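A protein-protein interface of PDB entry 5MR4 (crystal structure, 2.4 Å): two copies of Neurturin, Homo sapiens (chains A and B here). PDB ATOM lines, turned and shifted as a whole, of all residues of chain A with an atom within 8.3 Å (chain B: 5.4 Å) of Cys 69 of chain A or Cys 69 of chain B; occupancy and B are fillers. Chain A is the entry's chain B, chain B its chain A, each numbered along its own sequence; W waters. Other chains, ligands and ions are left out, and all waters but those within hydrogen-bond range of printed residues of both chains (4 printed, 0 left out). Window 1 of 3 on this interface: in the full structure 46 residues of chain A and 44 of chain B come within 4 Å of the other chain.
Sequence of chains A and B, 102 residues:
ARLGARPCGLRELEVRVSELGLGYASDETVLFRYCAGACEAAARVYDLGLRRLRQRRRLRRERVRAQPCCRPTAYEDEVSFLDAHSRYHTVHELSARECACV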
ATOM      1  N   CYS A   8     -12.066   0.305  23.143  1.00  0.00           N
ATOM      2  CA  CYS A   8     -13.330   0.239  22.412  1.00  0.00           C
ATOM      3  C   CYS A   8     -13.974   1.604  22.184  1.00  0.00           C
ATOM      4  O   CYS A   8     -14.184   2.355  23.109  1.00  0.00           O
ATOM      5  CB  CYS A   8     -14.313  -0.666  23.140  1.00  0.00           C
ATOM      6  SG  CYS A   8     -15.977  -0.760  22.402  1.00  0.00           S
ATOM      7  N   CYS A  35     -17.323   0.438  15.261  1.00  0.00           N
ATOM      8  CA  CYS A  35     -16.810   0.185  16.607  1.00  0.00           C
ATOM      9  C   CYS A  35     -15.600  -0.735  16.539  1.00  0.00           C
ATOM     10  O   CYS A  35     -15.654  -1.788  15.940  1.00  0.00           O
ATOM     11  CB  CYS A  35     -17.886  -0.442  17.494  1.00  0.00           C
ATOM     12  SG  CYS A  35     -19.315   0.635  17.730  1.00  0.00           S
ATOM     13  N   GLY A  37     -11.515  -1.578  18.737  1.00  0.00           N
ATOM     14  CA  GLY A  37     -10.710  -1.474  19.941  1.00  0.00           C
ATOM     15  C   GLY A  37     -10.962  -2.526  20.996  1.00  0.00           C
ATOM     16  O   GLY A  37     -11.861  -3.363  20.879  1.00  0.00           O
ATOM     17  N   ALA A  38     -10.145  -2.442  22.040  1.00  0.00           N
ATOM     18  CA  ALA A  38     -10.059  -3.446  23.104  1.00  0.00           C
ATOM     19  C   ALA A  38     -10.995  -3.102  24.256  1.00  0.00           C
ATOM     20  O   ALA A  38     -11.180  -1.935  24.601  1.00  0.00           O
ATOM     21  CB  ALA A  38      -8.632  -3.533  23.613  1.00  0.00           C
ATOM     22  N   CYS A  39     -11.599  -4.138  24.817  1.00  0.00           N
ATOM     23  CA  CYS A  39     -12.416  -4.036  26.015  1.00  0.00           C
ATOM     24  C   CYS A  39     -11.454  -4.303  27.164  1.00  0.00           C
ATOM     25  O   CYS A  39     -10.964  -5.398  27.312  1.00  0.00           O
ATOM     26  CB  CYS A  39     -13.552  -5.068  25.940  1.00  0.00           C
ATOM     27  SG  CYS A  39     -14.833  -4.629  24.707  1.00  0.00           S
ATOM     28  N   ASP A  47     -17.428 -14.324  33.480  1.00  0.00           N
ATOM     29  CA  ASP A  47     -16.536 -14.786  32.412  1.00  0.00           C
ATOM     30  C   ASP A  47     -15.443 -15.723  32.935  1.00  0.00           C
ATOM     31  O   ASP A  47     -15.103 -16.704  32.278  1.00  0.00           O
ATOM     32  CB  ASP A  47     -15.936 -13.600  31.657  1.00  0.00           C
ATOM     33  CG  ASP A  47     -16.944 -12.945  30.705  1.00  0.00           C
ATOM     34  OD1 ASP A  47     -17.724 -13.698  30.082  1.00  0.00           O
ATOM     35  OD2 ASP A  47     -16.967 -11.691  30.570  1.00  0.00           O
ATOM     36  N   ARG A  63     -21.446 -23.025  21.161  1.00  0.00           N
ATOM     37  CA  ARG A  63     -20.786 -21.731  21.003  1.00  0.00           C
ATOM     38  C   ARG A  63     -21.030 -20.829  22.221  1.00  0.00           C
ATOM     39  O   ARG A  63     -22.194 -20.510  22.552  1.00  0.00           O
ATOM     40  CB  ARG A  63     -21.277 -21.026  19.744  1.00  0.00           C
ATOM     41  CG  ARG A  63     -20.391 -19.870  19.316  1.00  0.00           C
ATOM     42  CD  ARG A  63     -21.105 -18.991  18.302  1.00  0.00           C
ATOM     43  NE  ARG A  63     -20.155 -18.167  17.549  1.00  0.00           N
ATOM     44  CZ  ARG A  63     -20.060 -18.097  16.216  1.00  0.00           C
ATOM     45  NH1 ARG A  63     -20.874 -18.795  15.409  1.00  0.00           N
ATOM     46  NH2 ARG A  63     -19.134 -17.306  15.676  1.00  0.00           N
ATOM     47  N   ARG A  65     -19.457 -17.192  24.138  1.00  0.00           N
ATOM     48  CA  ARG A  65     -18.612 -16.017  24.211  1.00  0.00           C
ATOM     49  C   ARG A  65     -18.319 -15.672  25.689  1.00  0.00           C
ATOM     50  O   ARG A  65     -19.210 -15.232  26.424  1.00  0.00           O
ATOM     51  CB  ARG A  65     -19.283 -14.852  23.506  1.00  0.00           C
ATOM     52  CG  ARG A  65     -18.369 -14.185  22.510  1.00  0.00           C
ATOM     53  CD  ARG A  65     -17.063 -13.723  23.153  1.00  0.00           C
ATOM     54  NE  ARG A  65     -16.515 -12.487  22.585  1.00  0.00           N
ATOM     55  CZ  ARG A  65     -15.430 -12.386  21.802  1.00  0.00           C
ATOM     56  NH1 ARG A  65     -14.714 -13.460  21.441  1.00  0.00           N
ATOM     57  NH2 ARG A  65     -15.041 -11.175  21.382  1.00  0.00           N
ATOM     58  N   ALA A  66     -17.065 -15.868  26.092  1.00  0.00           N
ATOM     59  CA  ALA A  66     -16.610 -15.735  27.465  1.00  0.00           C
ATOM     60  C   ALA A  66     -15.688 -14.540  27.637  1.00  0.00           C
ATOM     61  O   ALA A  66     -14.796 -14.528  28.503  1.00  0.00           O
ATOM     62  CB  ALA A  66     -15.919 -17.004  27.906  1.00  0.00           C
ATOM     63  N   GLN A  67     -15.992 -13.508  26.870  1.00  0.00           N
ATOM     64  CA  GLN A  67     -15.209 -12.285  26.797  1.00  0.00           C
ATOM     65  C   GLN A  67     -16.143 -11.170  26.333  1.00  0.00           C
ATOM     66  O   GLN A  67     -17.016 -11.427  25.537  1.00  0.00           O
ATOM     67  CB  GLN A  67     -14.202 -12.507  25.725  1.00  0.00           C
ATOM     68  CG  GLN A  67     -13.082 -11.532  25.729  1.00  0.00           C
ATOM     69  CD  GLN A  67     -12.150 -11.844  24.594  1.00  0.00           C
ATOM     70  OE1 GLN A  67     -12.253 -12.913  23.988  1.00  0.00           O
ATOM     71  NE2 GLN A  67     -11.255 -10.918  24.280  1.00  0.00           N
ATOM     72  N   PRO A  68     -15.972  -9.932  26.815  1.00  0.00           N
ATOM     73  CA  PRO A  68     -16.825  -8.890  26.253  1.00  0.00           C
ATOM     74  C   PRO A  68     -16.534  -8.598  24.770  1.00  0.00           C
ATOM     75  O   PRO A  68     -15.482  -8.957  24.268  1.00  0.00           O
ATOM     76  CB  PRO A  68     -16.512  -7.675  27.118  1.00  0.00           C
ATOM     77  CG  PRO A  68     -15.841  -8.189  28.336  1.00  0.00           C
ATOM     78  CD  PRO A  68     -15.142  -9.431  27.920  1.00  0.00           C
ATOM     79  N   CYS A  69     -17.492  -7.966  24.091  1.00  0.00           N
ATOM     80  CA  CYS A  69     -17.383  -7.613  22.674  1.00  0.00           C
ATOM     81  C   CYS A  69     -17.612  -6.143  22.510  1.00  0.00           C
ATOM     82  O   CYS A  69     -18.524  -5.603  23.113  1.00  0.00           O
ATOM     83  CB  CYS A  69     -18.443  -8.329  21.831  1.00  0.00           C
ATOM     84  SG  CYS A  69     -18.271 -10.110  21.669  1.00  0.00           S
ATOM     85  N   CYS A  70     -16.783  -5.509  21.686  1.00  0.00           N
ATOM     86  CA  CYS A  70     -16.942  -4.119  21.314  1.00  0.00           C
ATOM     87  C   CYS A  70     -17.882  -4.101  20.100  1.00  0.00           C
ATOM     88  O   CYS A  70     -17.506  -4.541  19.009  1.00  0.00           O
ATOM     89  CB  CYS A  70     -15.600  -3.510  20.956  1.00  0.00           C
ATOM     90  SG  CYS A  70     -15.697  -1.746  20.561  1.00  0.00           S
ATOM     91  N   ARG A  71     -19.101  -3.622  20.318  1.00  0.00           N
ATOM     92  CA  ARG A  71     -20.139  -3.641  19.307  1.00  0.00           C
ATOM     93  C   ARG A  71     -21.021  -2.395  19.378  1.00  0.00           C
ATOM     94  O   ARG A  71     -21.084  -1.721  20.399  1.00  0.00           O
ATOM     95  CB  ARG A  71     -21.024  -4.879  19.460  1.00  0.00           C
ATOM     96  CG  ARG A  71     -20.411  -6.211  19.090  1.00  0.00           C
ATOM     97  CD  ARG A  71     -20.302  -6.395  17.591  1.00  0.00           C
ATOM     98  NE  ARG A  71     -21.583  -6.497  16.878  1.00  0.00           N
ATOM     99  CZ  ARG A  71     -21.717  -6.483  15.539  1.00  0.00           C
ATOM    100  NH1 ARG A  71     -20.654  -6.373  14.720  1.00  0.00           N
ATOM    101  NH2 ARG A  71     -22.922  -6.605  15.000  1.00  0.00           N
ATOM    102  N   PRO A  72     -21.714  -2.068  18.279  1.00  0.00           N
ATOM    103  CA  PRO A  72     -22.568  -0.878  18.347  1.00  0.00           C
ATOM    104  C   PRO A  72     -23.782  -1.059  19.249  1.00  0.00           C
ATOM    105  O   PRO A  72     -24.375  -2.112  19.258  1.00  0.00           O
ATOM    106  CB  PRO A  72     -22.984  -0.659  16.894  1.00  0.00           C
ATOM    107  CG  PRO A  72     -21.973  -1.382  16.077  1.00  0.00           C
ATOM    108  CD  PRO A  72     -21.543  -2.551  16.900  1.00  0.00           C
ATOM    109  N   THR A  73     -24.118  -0.042  20.018  1.00  0.00           N
ATOM    110  CA  THR A  73     -25.386  -0.005  20.776  1.00  0.00           C
ATOM    111  C   THR A  73     -26.468   0.765  20.002  1.00  0.00           C
ATOM    112  O   THR A  73     -27.638   0.723  20.349  1.00  0.00           O
ATOM    113  CB  THR A  73     -25.196   0.672  22.166  1.00  0.00           C
ATOM    114  OG1 THR A  73     -24.613   1.969  21.983  1.00  0.00           O
ATOM    115  CG2 THR A  73     -24.257  -0.131  23.006  1.00  0.00           C
ATOM    116  N   CYS A  99     -21.004   2.962  20.732  1.00  0.00           N
ATOM    117  CA  CYS A  99     -20.299   1.710  20.988  1.00  0.00           C
ATOM    118  C   CYS A  99     -20.310   1.383  22.465  1.00  0.00           C
ATOM    119  O   CYS A  99     -20.394   2.261  23.274  1.00  0.00           O
ATOM    120  CB  CYS A  99     -18.840   1.819  20.565  1.00  0.00           C
ATOM    121  SG  CYS A  99     -18.660   2.270  18.824  1.00  0.00           S
ATOM    122  N   ALA A 100     -20.210   0.102  22.790  1.00  0.00           N
ATOM    123  CA  ALA A 100     -20.067  -0.351  24.175  1.00  0.00           C
ATOM    124  C   ALA A 100     -19.413  -1.723  24.155  1.00  0.00           C
ATOM    125  O   ALA A 100     -19.401  -2.408  23.114  1.00  0.00           O
ATOM    126  CB  ALA A 100     -21.415  -0.418  24.873  1.00  0.00           C
ATOM    127  N   CYS A 101     -18.851  -2.085  25.301  1.00  0.00           N
ATOM    128  CA  CYS A 101     -18.295  -3.396  25.550  1.00  0.00           C
ATOM    129  C   CYS A 101     -19.360  -4.109  26.322  1.00  0.00           C
ATOM    130  O   CYS A 101     -19.751  -3.639  27.382  1.00  0.00           O
ATOM    131  CB  CYS A 101     -17.025  -3.298  26.402  1.00  0.00           C
ATOM    132  SG  CYS A 101     -15.572  -2.789  25.446  1.00  0.00           S
ATOM    133  N   VAL A 102     -19.831  -5.233  25.791  1.00  0.00           N
ATOM    134  CA  VAL A 102     -20.870  -6.028  26.424  1.00  0.00           C
ATOM    135  C   VAL A 102     -20.402  -7.474  26.520  1.00  0.00           C
ATOM    136  O   VAL A 102     -20.453  -8.089  27.588  1.00  0.00           O
ATOM    137  CB  VAL A 102     -22.229  -5.936  25.672  1.00  0.00           C
ATOM    138  CG1 VAL A 102     -22.964  -4.680  26.108  1.00  0.00           C
ATOM    139  CG2 VAL A 102     -22.047  -5.922  24.155  1.00  0.00           C
ATOM    140  OXT VAL A 102     -19.978  -8.062  25.518  1.00  0.00           O
ATOM    141  N   CYS B  39     -26.321 -16.525  16.933  1.00  0.00           N
ATOM    142  CA  CYS B  39     -27.031 -15.339  16.545  1.00  0.00           C
ATOM    143  C   CYS B  39     -27.443 -15.567  15.087  1.00  0.00           C
ATOM    144  O   CYS B  39     -26.597 -15.613  14.211  1.00  0.00           O
ATOM    145  CB  CYS B  39     -26.097 -14.129  16.675  1.00  0.00           C
ATOM    146  SG  CYS B  39     -25.725 -13.678  18.403  1.00  0.00           S
ATOM    147  N   ARG B  65     -14.905  -6.383  15.633  1.00  0.00           N
ATOM    148  CA  ARG B  65     -15.906  -7.455  15.654  1.00  0.00           C
ATOM    149  C   ARG B  65     -16.971  -7.187  14.575  1.00  0.00           C
ATOM    150  O   ARG B  65     -17.793  -6.285  14.715  1.00  0.00           O
ATOM    151  CB  ARG B  65     -16.524  -7.558  17.063  1.00  0.00           C
ATOM    152  CG  ARG B  65     -16.606  -8.961  17.601  1.00  0.00           C
ATOM    153  CD  ARG B  65     -17.346  -9.889  16.648  1.00  0.00           C
ATOM    154  NE  ARG B  65     -18.084 -10.983  17.291  1.00  0.00           N
ATOM    155  CZ  ARG B  65     -17.727 -12.279  17.316  1.00  0.00           C
ATOM    156  NH1 ARG B  65     -16.596 -12.711  16.743  1.00  0.00           N
ATOM    157  NH2 ARG B  65     -18.524 -13.171  17.923  1.00  0.00           N
ATOM    158  N   GLN B  67     -19.486  -9.202  13.505  1.00  0.00           N
ATOM    159  CA  GLN B  67     -20.449 -10.268  13.650  1.00  0.00           C
ATOM    160  C   GLN B  67     -21.101 -10.061  15.000  1.00  0.00           C
ATOM    161  O   GLN B  67     -20.417  -9.686  15.923  1.00  0.00           O
ATOM    162  CB  GLN B  67     -19.666 -11.527  13.697  1.00  0.00           C
ATOM    163  CG  GLN B  67     -20.517 -12.734  13.656  1.00  0.00           C
ATOM    164  CD  GLN B  67     -19.684 -13.956  13.830  1.00  0.00           C
ATOM    165  OE1 GLN B  67     -18.457 -13.881  13.833  1.00  0.00           O
ATOM    166  NE2 GLN B  67     -20.338 -15.091  13.966  1.00  0.00           N
ATOM    167  N   PRO B  68     -22.411 -10.301  15.138  1.00  0.00           N
ATOM    168  CA  PRO B  68     -22.980 -10.111  16.480  1.00  0.00           C
ATOM    169  C   PRO B  68     -22.451 -11.103  17.519  1.00  0.00           C
ATOM    170  O   PRO B  68     -21.886 -12.132  17.156  1.00  0.00           O
ATOM    171  CB  PRO B  68     -24.473 -10.308  16.258  1.00  0.00           C
ATOM    172  CG  PRO B  68     -24.698 -10.126  14.802  1.00  0.00           C
ATOM    173  CD  PRO B  68     -23.452 -10.601  14.136  1.00  0.00           C
ATOM    174  N   CYS B  69     -22.629 -10.780  18.798  1.00  0.00           N
ATOM    175  CA  CYS B  69     -22.206 -11.651  19.896  1.00  0.00           C
ATOM    176  C   CYS B  69     -23.386 -11.962  20.783  1.00  0.00           C
ATOM    177  O   CYS B  69     -24.190 -11.099  21.069  1.00  0.00           O
ATOM    178  CB  CYS B  69     -21.140 -10.981  20.782  1.00  0.00           C
ATOM    179  SG  CYS B  69     -19.550 -10.592  20.023  1.00  0.00           S
ATOM    180  N   CYS B  70     -23.448 -13.193  21.255  1.00  0.00           N
ATOM    181  CA  CYS B  70     -24.406 -13.596  22.242  1.00  0.00           C
ATOM    182  C   CYS B  70     -23.782 -13.326  23.622  1.00  0.00           C
ATOM    183  O   CYS B  70     -22.856 -14.033  24.046  1.00  0.00           O
ATOM    184  CB  CYS B  70     -24.725 -15.072  22.079  1.00  0.00           C
ATOM    185  SG  CYS B  70     -26.013 -15.650  23.192  1.00  0.00           S
ATOM    186  N   ARG B  71     -24.315 -12.317  24.306  1.00  0.00           N
ATOM    187  CA  ARG B  71     -23.787 -11.863  25.581  1.00  0.00           C
ATOM    188  C   ARG B  71     -24.900 -11.478  26.534  1.00  0.00           C
ATOM    189  O   ARG B  71     -26.003 -11.189  26.104  1.00  0.00           O
ATOM    190  CB  ARG B  71     -22.838 -10.680  25.386  1.00  0.00           C
ATOM    191  CG  ARG B  71     -21.508 -11.029  24.723  1.00  0.00           C
ATOM    192  CD  ARG B  71     -20.575 -11.769  25.675  1.00  0.00           C
ATOM    193  NE  ARG B  71     -20.122 -10.971  26.812  1.00  0.00           N
ATOM    194  CZ  ARG B  71     -19.415 -11.454  27.845  1.00  0.00           C
ATOM    195  NH1 ARG B  71     -19.092 -12.744  27.911  1.00  0.00           N
ATOM    196  NH2 ARG B  71     -19.026 -10.645  28.831  1.00  0.00           N
ATOM    197  N   ALA B 100     -28.786 -11.396  24.809  1.00  0.00           N
ATOM    198  CA  ALA B 100     -29.133 -10.765  23.550  1.00  0.00           C
ATOM    199  C   ALA B 100     -27.978 -10.900  22.580  1.00  0.00           C
ATOM    200  O   ALA B 100     -26.826 -11.117  22.980  1.00  0.00           O
ATOM    201  CB  ALA B 100     -29.448  -9.300  23.760  1.00  0.00           C
ATOM    202  N   CYS B 101     -28.295 -10.771  21.301  1.00  0.00           N
ATOM    203  CA  CYS B 101     -27.277 -10.709  20.266  1.00  0.00           C
ATOM    204  C   CYS B 101     -27.060  -9.265  19.926  1.00  0.00           C
ATOM    205  O   CYS B 101     -27.991  -8.584  19.566  1.00  0.00           O
ATOM    206  CB  CYS B 101     -27.724 -11.461  19.048  1.00  0.00           C
ATOM    207  SG  CYS B 101     -27.639 -13.249  19.174  1.00  0.00           S
ATOM    208  N   VAL B 102     -25.828  -8.802  20.031  1.00  0.00           N
ATOM    209  CA  VAL B 102     -25.499  -7.402  19.790  1.00  0.00           C
ATOM    210  C   VAL B 102     -24.333  -7.356  18.802  1.00  0.00           C
ATOM    211  O   VAL B 102     -24.364  -6.662  17.781  1.00  0.00           O
ATOM    212  CB  VAL B 102     -25.105  -6.673  21.103  1.00  0.00           C
ATOM    213  CG1 VAL B 102     -25.120  -5.163  20.920  1.00  0.00           C
ATOM    214  CG2 VAL B 102     -26.058  -7.035  22.219  1.00  0.00           C
ATOM    215  OXT VAL B 102     -23.326  -8.026  19.035  1.00  0.00           O
HETATM  216  O   HOH W   1     -22.296 -16.667  24.219  1.00  0.00           O
HETATM  217  O   HOH W   2     -18.137  -3.528  15.413  1.00  0.00           O
HETATM  218  O   HOH W   3     -15.391  -4.284  17.326  1.00  0.00           O
HETATM  219  O   HOH W   4     -25.150  -4.111  17.488  1.00  0.00           O
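Of the 20 printed residues of chain A, 11 touch a printed residue of chain B.
Printed residues of chain B that touch a printed residue of chain A: Arg 65, Gln 67, Pro 68, Cys 69, Cys 70, Arg 71 and Val 102.
Hydrophobic or aromatic side chains of chain B that line the printed part of chain A: Pro 68 and Val 102.
Among the printed residues, 15 pairs touch across the chains.
OXT of Val 102 of chain A lies within hydrogen-bond range of N of Cys 69 of chain A (2.9 Å).
The guanidinium group of Arg 65 of chain B is in hydrogen-bond range of the backbone carbonyl oxygen of Gln 67 of chain B (3.0 Å).
SG of Cys 101 of chain A is disulfide-bonded to SG of Cys 39 of chain A (2.1 Å).
The side-chain sulfur of Cys 8 of chain A is disulfide-bonded to the side-chain sulfur of Cys 70 of chain A, 2.1 Å away.
N of Cys 70 of chain A sits at hydrogen-bond distance from SG of Cys 39 of chain A (3.7 Å).
SG of Cys 39 of chain B is in hydrogen-bond range of N of Cys 70 of chain B (3.7 Å).
Cys 70 of chain B touches Arg 65 of chain A (O to CB, 3.7 Å).
Arg 71 of chain B touches Ala 66 of chain A.
N of Pro 68 of chain A touches NH2 of Arg 71 of chain B (3.7 Å).
Arg 65 of chain B touches Cys 70 of chain A.
NH2 of Arg 71 of chain A touches N of Pro 68 of chain B, 3.7 Å away.
Val 102 of chain B touches Pro 72 of chain A (CG1 to O, 3.6 Å).
The guanidinium group (NH1) of Arg 71 of chain B lies within salt-bridge range of the side-chain carboxylate (OD1) of Asp 47 of chain A, at 2.7 Å.
The side-chain sulfur of Cys 69 of chain A forms a disulfide with the side-chain sulfur of Cys 69 of chain B, 2.1 Å away.
The chain-end carboxylate (O) of Val 102 of chain B lies within salt-bridge range of the guanidinium group (NE) of Arg 71 of chain A (2.9 Å).
O of Val 102 of chain A lies within salt-bridge range of NE of Arg 71 of chain B (3.0 Å).
N of Gln 67 of chain B lies close to NH1 of Arg 71 of chain A, at 3.3 Å.
The backbone carbonyl oxygen of Arg 65 of chain B lies within hydrogen-bond range of the guanidinium group of Arg 71 of chain A (2.9 Å).
The backbone carbonyl oxygen of Gln 67 of chain A sits close to the guanidinium group of Arg 71 of chain B.
The guanidinium group (NH1) of Arg 71 of chain B is in hydrogen-bond range of the backbone carbonyl oxygen (O) of Arg 65 of chain A.
NE2 of Gln 67 of chain B lies close to NH2 of Arg 63 of chain A (3.0 Å).
Water W4 lies within hydrogen-bond range of the chain-end carboxylate (O) of Val 102 of chain B (2.7 Å) and the backbone carbonyl oxygen (O) of Pro 72 of chain A (2.8 Å).
Water W1 bridges O of Cys 70 of chain B and N of Arg 65 of chain A.
Water W3 lies within hydrogen-bond range of the backbone carbonyl oxygen (O) of Cys 70 of chain A (2.7 Å), the backbone NH (N) of Arg 65 of chain B (2.7 Å) and the backbone carbonyl oxygen (O) of Cys 35 of chain A (2.9 Å).
Water W2 lies within hydrogen-bond range of the backbone carbonyl oxygen (O) of Arg 65 of chain B (2.9 Å) and the backbone carbonyl oxygen (O) of Cys 35 of chain A (3.1 Å).
Gln 67 of chain A touches Arg 71 of chain B, and with the chains exchanged Arg 71 of chain A touches Gln 67 of chain B.
Pro 68 of chain A touches Arg 71 of chain B, and with the chains exchanged Arg 71 of chain A touches Pro 68 of chain B.
Cys 69 of chain A touches its own counterpart, Cys 69 of chain B.
Arg 71 of chain A touches Val 102 of chain B, and with the chains exchanged Val 102 of chain A touches Arg 71 of chain B.
Positions printed for both chains: 39, 65, 67, 68, 69, 70, 71, 100, 101 and 102.
Of the 15 pairs that touch across the chains among the printed residues, 11 have their exchanged pair printed and touching as well.
Of the printed residues of chain B, Pro 68 of chain A touches Arg 71.
Printed residues of chain B within 4 Å of Cys 69 of chain A: Cys 69.
Of the printed residues of chain B, Arg 71 of chain A touches Arg 65 (2.9 Å), Gln 67 (3.3 Å), Pro 68 (3.7 Å) and Val 102 (2.9 Å).
Ala 100 of chain A touches none of the printed residues of chain B.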
